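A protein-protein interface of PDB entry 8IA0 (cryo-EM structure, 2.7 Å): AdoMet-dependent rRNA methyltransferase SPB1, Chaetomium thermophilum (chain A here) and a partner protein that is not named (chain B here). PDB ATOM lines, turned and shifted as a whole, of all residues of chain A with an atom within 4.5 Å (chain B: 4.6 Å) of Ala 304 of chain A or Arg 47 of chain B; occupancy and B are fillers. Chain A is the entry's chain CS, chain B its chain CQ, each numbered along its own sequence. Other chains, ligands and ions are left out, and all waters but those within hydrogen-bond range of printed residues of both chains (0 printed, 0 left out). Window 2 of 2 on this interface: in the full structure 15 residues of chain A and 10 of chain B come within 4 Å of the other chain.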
ATOM      1  N   LYS A 300     -16.753   2.469 -28.637  1.00  0.00           N
ATOM      2  CA  LYS A 300     -16.080   3.632 -29.202  1.00  0.00           C
ATOM      3  C   LYS A 300     -14.589   3.610 -28.889  1.00  0.00           C
ATOM      4  O   LYS A 300     -13.766   4.008 -29.721  1.00  0.00           O
ATOM      5  CB  LYS A 300     -16.720   4.916 -28.678  1.00  0.00           C
ATOM      6  CG  LYS A 300     -17.002   5.947 -29.754  1.00  0.00           C
ATOM      7  CD  LYS A 300     -17.414   7.275 -29.151  1.00  0.00           C
ATOM      8  CE  LYS A 300     -16.301   7.861 -28.300  1.00  0.00           C
ATOM      9  NZ  LYS A 300     -16.558   9.287 -27.964  1.00  0.00           N
ATOM     10  N   GLU A 301     -14.224   3.155 -27.688  1.00  0.00           N
ATOM     11  CA  GLU A 301     -12.814   3.078 -27.323  1.00  0.00           C
ATOM     12  C   GLU A 301     -12.067   2.094 -28.211  1.00  0.00           C
ATOM     13  O   GLU A 301     -10.898   2.313 -28.550  1.00  0.00           O
ATOM     14  CB  GLU A 301     -12.672   2.685 -25.852  1.00  0.00           C
ATOM     15  CG  GLU A 301     -13.028   3.793 -24.875  1.00  0.00           C
ATOM     16  CD  GLU A 301     -12.051   4.952 -24.927  1.00  0.00           C
ATOM     17  OE1 GLU A 301     -10.853   4.711 -25.186  1.00  0.00           O
ATOM     18  OE2 GLU A 301     -12.481   6.104 -24.710  1.00  0.00           O
ATOM     19  N   ILE A 302     -12.724   0.997 -28.592  1.00  0.00           N
ATOM     20  CA  ILE A 302     -12.081   0.008 -29.451  1.00  0.00           C
ATOM     21  C   ILE A 302     -11.787   0.601 -30.822  1.00  0.00           C
ATOM     22  O   ILE A 302     -10.709   0.389 -31.390  1.00  0.00           O
ATOM     23  CB  ILE A 302     -12.953  -1.255 -29.549  1.00  0.00           C
ATOM     24  CG1 ILE A 302     -12.918  -2.009 -28.220  1.00  0.00           C
ATOM     25  CG2 ILE A 302     -12.499  -2.139 -30.702  1.00  0.00           C
ATOM     26  CD1 ILE A 302     -11.777  -2.984 -28.104  1.00  0.00           C
ATOM     27  N   ARG A 303     -12.735   1.362 -31.370  1.00  0.00           N
ATOM     28  CA  ARG A 303     -12.530   1.963 -32.682  1.00  0.00           C
ATOM     29  C   ARG A 303     -11.475   3.063 -32.630  1.00  0.00           C
ATOM     30  O   ARG A 303     -10.770   3.303 -33.617  1.00  0.00           O
ATOM     31  CB  ARG A 303     -13.854   2.502 -33.218  1.00  0.00           C
ATOM     32  CG  ARG A 303     -14.926   1.438 -33.359  1.00  0.00           C
ATOM     33  CD  ARG A 303     -16.149   1.976 -34.077  1.00  0.00           C
ATOM     34  NE  ARG A 303     -15.869   2.316 -35.467  1.00  0.00           N
ATOM     35  CZ  ARG A 303     -15.776   1.433 -36.451  1.00  0.00           C
ATOM     36  NH1 ARG A 303     -15.929   0.138 -36.233  1.00  0.00           N
ATOM     37  NH2 ARG A 303     -15.526   1.860 -37.685  1.00  0.00           N
ATOM     38  N   ALA A 304     -11.359   3.748 -31.492  1.00  0.00           N
ATOM     39  CA  ALA A 304     -10.326   4.769 -31.346  1.00  0.00           C
ATOM     40  C   ALA A 304      -8.929   4.160 -31.390  1.00  0.00           C
ATOM     41  O   ALA A 304      -8.025   4.706 -32.033  1.00  0.00           O
ATOM     42  CB  ALA A 304     -10.532   5.542 -30.044  1.00  0.00           C
ATOM     43  N   CYS A 305      -8.732   3.029 -30.706  1.00  0.00           N
ATOM     44  CA  CYS A 305      -7.416   2.399 -30.679  1.00  0.00           C
ATOM     45  C   CYS A 305      -7.036   1.842 -32.044  1.00  0.00           C
ATOM     46  O   CYS A 305      -5.871   1.915 -32.451  1.00  0.00           O
ATOM     47  CB  CYS A 305      -7.386   1.295 -29.624  1.00  0.00           C
ATOM     48  SG  CYS A 305      -7.663   1.859 -27.933  1.00  0.00           S
ATOM     49  N   CYS A 306      -8.006   1.275 -32.765  1.00  0.00           N
ATOM     50  CA  CYS A 306      -7.710   0.665 -34.058  1.00  0.00           C
ATOM     51  C   CYS A 306      -7.299   1.711 -35.085  1.00  0.00           C
ATOM     52  O   CYS A 306      -6.549   1.412 -36.022  1.00  0.00           O
ATOM     53  CB  CYS A 306      -8.922  -0.124 -34.553  1.00  0.00           C
ATOM     54  SG  CYS A 306      -9.089  -1.768 -33.826  1.00  0.00           S
ATOM     55  N   ASP A 307      -7.787   2.943 -34.933  1.00  0.00           N
ATOM     56  CA  ASP A 307      -7.462   3.991 -35.893  1.00  0.00           C
ATOM     57  C   ASP A 307      -5.987   4.370 -35.826  1.00  0.00           C
ATOM     58  O   ASP A 307      -5.362   4.644 -36.857  1.00  0.00           O
ATOM     59  CB  ASP A 307      -8.345   5.213 -35.644  1.00  0.00           C
ATOM     60  CG  ASP A 307      -8.792   5.880 -36.929  1.00  0.00           C
ATOM     61  OD1 ASP A 307      -7.974   6.593 -37.546  1.00  0.00           O
ATOM     62  OD2 ASP A 307      -9.962   5.689 -37.321  1.00  0.00           O
ATOM     63  N   ASP A 308      -5.413   4.393 -34.620  1.00  0.00           N
ATOM     64  CA  ASP A 308      -4.024   4.805 -34.399  1.00  0.00           C
ATOM     65  C   ASP A 308      -3.365   3.769 -33.491  1.00  0.00           C
ATOM     66  O   ASP A 308      -3.543   3.789 -32.271  1.00  0.00           O
ATOM     67  CB  ASP A 308      -3.964   6.210 -33.802  1.00  0.00           C
ATOM     68  CG  ASP A 308      -2.801   7.023 -34.335  1.00  0.00           C
ATOM     69  OD1 ASP A 308      -1.722   6.439 -34.567  1.00  0.00           O
ATOM     70  OD2 ASP A 308      -2.966   8.246 -34.521  1.00  0.00           O
ATOM     71  N   ASN B  45      -3.517   7.776 -22.531  1.00  0.00           N
ATOM     72  CA  ASN B  45      -4.722   7.889 -23.338  1.00  0.00           C
ATOM     73  C   ASN B  45      -5.399   9.217 -23.044  1.00  0.00           C
ATOM     74  O   ASN B  45      -5.898   9.410 -21.925  1.00  0.00           O
ATOM     75  CB  ASN B  45      -5.672   6.732 -23.046  1.00  0.00           C
ATOM     76  CG  ASN B  45      -6.558   6.398 -24.222  1.00  0.00           C
ATOM     77  OD1 ASN B  45      -6.730   7.207 -25.131  1.00  0.00           O
ATOM     78  ND2 ASN B  45      -7.132   5.202 -24.212  1.00  0.00           N
ATOM     79  N   PRO B  46      -5.436  10.158 -23.990  1.00  0.00           N
ATOM     80  CA  PRO B  46      -6.149  11.419 -23.734  1.00  0.00           C
ATOM     81  C   PRO B  46      -7.628  11.222 -23.458  1.00  0.00           C
ATOM     82  O   PRO B  46      -8.238  12.056 -22.777  1.00  0.00           O
ATOM     83  CB  PRO B  46      -5.912  12.225 -25.020  1.00  0.00           C
ATOM     84  CG  PRO B  46      -5.505  11.221 -26.044  1.00  0.00           C
ATOM     85  CD  PRO B  46      -4.778  10.150 -25.305  1.00  0.00           C
ATOM     86  N   ARG B  47      -8.223  10.142 -23.966  1.00  0.00           N
ATOM     87  CA  ARG B  47      -9.620   9.850 -23.677  1.00  0.00           C
ATOM     88  C   ARG B  47      -9.842   9.458 -22.223  1.00  0.00           C
ATOM     89  O   ARG B  47     -10.971   9.557 -21.733  1.00  0.00           O
ATOM     90  CB  ARG B  47     -10.123   8.736 -24.594  1.00  0.00           C
ATOM     91  CG  ARG B  47     -10.471   9.193 -25.996  1.00  0.00           C
ATOM     92  CD  ARG B  47     -10.287   8.073 -27.000  1.00  0.00           C
ATOM     93  NE  ARG B  47      -9.007   8.161 -27.692  1.00  0.00           N
ATOM     94  CZ  ARG B  47      -8.167   7.146 -27.843  1.00  0.00           C
ATOM     95  NH1 ARG B  47      -8.439   5.946 -27.358  1.00  0.00           N
ATOM     96  NH2 ARG B  47      -7.025   7.342 -28.496  1.00  0.00           N
ATOM     97  N   LYS B  48      -8.798   9.016 -21.526  1.00  0.00           N
ATOM     98  CA  LYS B  48      -8.915   8.601 -20.135  1.00  0.00           C
ATOM     99  C   LYS B  48      -8.524   9.689 -19.148  1.00  0.00           C
ATOM    100  O   LYS B  48      -9.023   9.691 -18.018  1.00  0.00           O
ATOM    101  CB  LYS B  48      -8.053   7.360 -19.881  1.00  0.00           C
ATOM    102  CG  LYS B  48      -8.580   6.086 -20.523  1.00  0.00           C
ATOM    103  CD  LYS B  48     -10.099   6.042 -20.528  1.00  0.00           C
ATOM    104  CE  LYS B  48     -10.610   4.617 -20.397  1.00  0.00           C
ATOM    105  NZ  LYS B  48     -11.419   4.206 -21.578  1.00  0.00           N
ATOM    106  N   LEU B  49      -7.647  10.609 -19.541  1.00  0.00           N
ATOM    107  CA  LEU B  49      -7.258  11.699 -18.659  1.00  0.00           C
ATOM    108  C   LEU B  49      -8.364  12.746 -18.614  1.00  0.00           C
ATOM    109  O   LEU B  49      -8.868  13.177 -19.655  1.00  0.00           O
ATOM    110  CB  LEU B  49      -5.945  12.318 -19.135  1.00  0.00           C
ATOM    111  CG  LEU B  49      -4.722  11.397 -19.097  1.00  0.00           C
ATOM    112  CD1 LEU B  49      -3.438  12.199 -19.095  1.00  0.00           C
ATOM    113  CD2 LEU B  49      -4.772  10.478 -17.888  1.00  0.00           C
ATOM    114  N   ALA B  54     -10.972  15.436 -25.075  1.00  0.00           N
ATOM    115  CA  ALA B  54     -11.372  14.109 -25.532  1.00  0.00           C
ATOM    116  C   ALA B  54     -12.199  13.391 -24.472  1.00  0.00           C
ATOM    117  O   ALA B  54     -13.213  12.757 -24.783  1.00  0.00           O
ATOM    118  CB  ALA B  54     -10.138  13.289 -25.902  1.00  0.00           C
ATOM    119  N   TYR B  55     -11.777  13.479 -23.209  1.00  0.00           N
ATOM    120  CA  TYR B  55     -12.561  12.893 -22.128  1.00  0.00           C
ATOM    121  C   TYR B  55     -13.877  13.633 -21.939  1.00  0.00           C
ATOM    122  O   TYR B  55     -14.931  13.008 -21.784  1.00  0.00           O
ATOM    123  CB  TYR B  55     -11.750  12.897 -20.832  1.00  0.00           C
ATOM    124  CG  TYR B  55     -12.535  12.519 -19.593  1.00  0.00           C
ATOM    125  CD1 TYR B  55     -12.629  11.197 -19.187  1.00  0.00           C
ATOM    126  CD2 TYR B  55     -13.164  13.486 -18.820  1.00  0.00           C
ATOM    127  CE1 TYR B  55     -13.339  10.847 -18.057  1.00  0.00           C
ATOM    128  CE2 TYR B  55     -13.877  13.145 -17.693  1.00  0.00           C
ATOM    129  CZ  TYR B  55     -13.961  11.824 -17.314  1.00  0.00           C
ATOM    130  OH  TYR B  55     -14.667  11.479 -16.188  1.00  0.00           O
ATOM    131  N   ASN B  58     -16.390  12.777 -24.704  1.00  0.00           N
ATOM    132  CA  ASN B  58     -16.839  11.392 -24.659  1.00  0.00           C
ATOM    133  C   ASN B  58     -17.544  11.025 -23.359  1.00  0.00           C
ATOM    134  O   ASN B  58     -18.164   9.958 -23.294  1.00  0.00           O
ATOM    135  CB  ASN B  58     -15.648  10.457 -24.973  1.00  0.00           C
ATOM    136  CG  ASN B  58     -14.849   9.998 -23.737  1.00  0.00           C
ATOM    137  OD1 ASN B  58     -15.149  10.318 -22.588  1.00  0.00           O
ATOM    138  ND2 ASN B  58     -13.805   9.222 -24.002  1.00  0.00           N
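NH1 of Arg 47 of chain B lies within salt-bridge range of OE1 of Glu 301 of chain A (3.5 Å). The side-chain amino group of Lys 48 of chain B lies within salt-bridge range of the side-chain carboxylate of Glu 301 of chain A. The side-chain amide nitrogen (ND2) of Asn 58 of chain B lies within hydrogen-bond range of the side-chain carboxylate (OE2) of Glu 301 of chain A, 3.5 Å away.
The guanidinium group of Arg 47 of chain B sits close to the side-chain amide oxygen of Asn 45 of chain B (3.1 Å). OD1 of Asn 58 of chain B sits close to O of Tyr 55 of chain B (2.8 Å). SG of Cys 305 of chain A is in hydrogen-bond range of O of Glu 301 of chain A, at 3.3 Å.
Among the printed residues, merely in contact across the chains: Lys 300 of chain A with Asn 58 of chain B, Ala 304 of chain A with Arg 47 of chain B and Glu 301 of chain A with Asn 45 of chain B.
Of chain B, only Arg 47 comes within 4 Å of Ala 304 of chain A. Of chain A, only Glu 301 (3.5 Å) and Ala 304 (3.4 Å) come within 4 Å of Arg 47 of chain B. Printed residues of chain A within 4 Å of Asn 45 of chain B: Glu 301. Of the printed residues of chain B, Glu 301 of chain A touches Asn 45 (3.9 Å), Arg 47 (3.5 Å), Lys 48 (3.5 Å) and Asn 58 (3.5 Å). Of the printed residues of chain B, Lys 300 of chain A touches Asn 58 (3.3 Å). Arg 303 of chain A touches none of the printed residues of chain B. Pro 46 of chain B touches none of the printed residues of chain A. The nearest printed residue of chain B that does not touch Glu 301 of chain A is Ala 54 of chain B (6.7 Å).
Of the 9 printed residues of chain A, 3 touch a printed residue of chain B. Of the 8 printed residues of chain B, 4 touch a printed residue of chain A. Among the printed residues, 6 pairs touch across the chains. Among the printed residues, Asp or Glu carboxylates within 4 Å of a Lys or Arg side-chain nitrogen of the other chain: Glu 301 of chain A with Arg 47 of chain B (3.5 Å) and Glu 301 of chain A with Lys 48 of chain B (3.7 Å).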
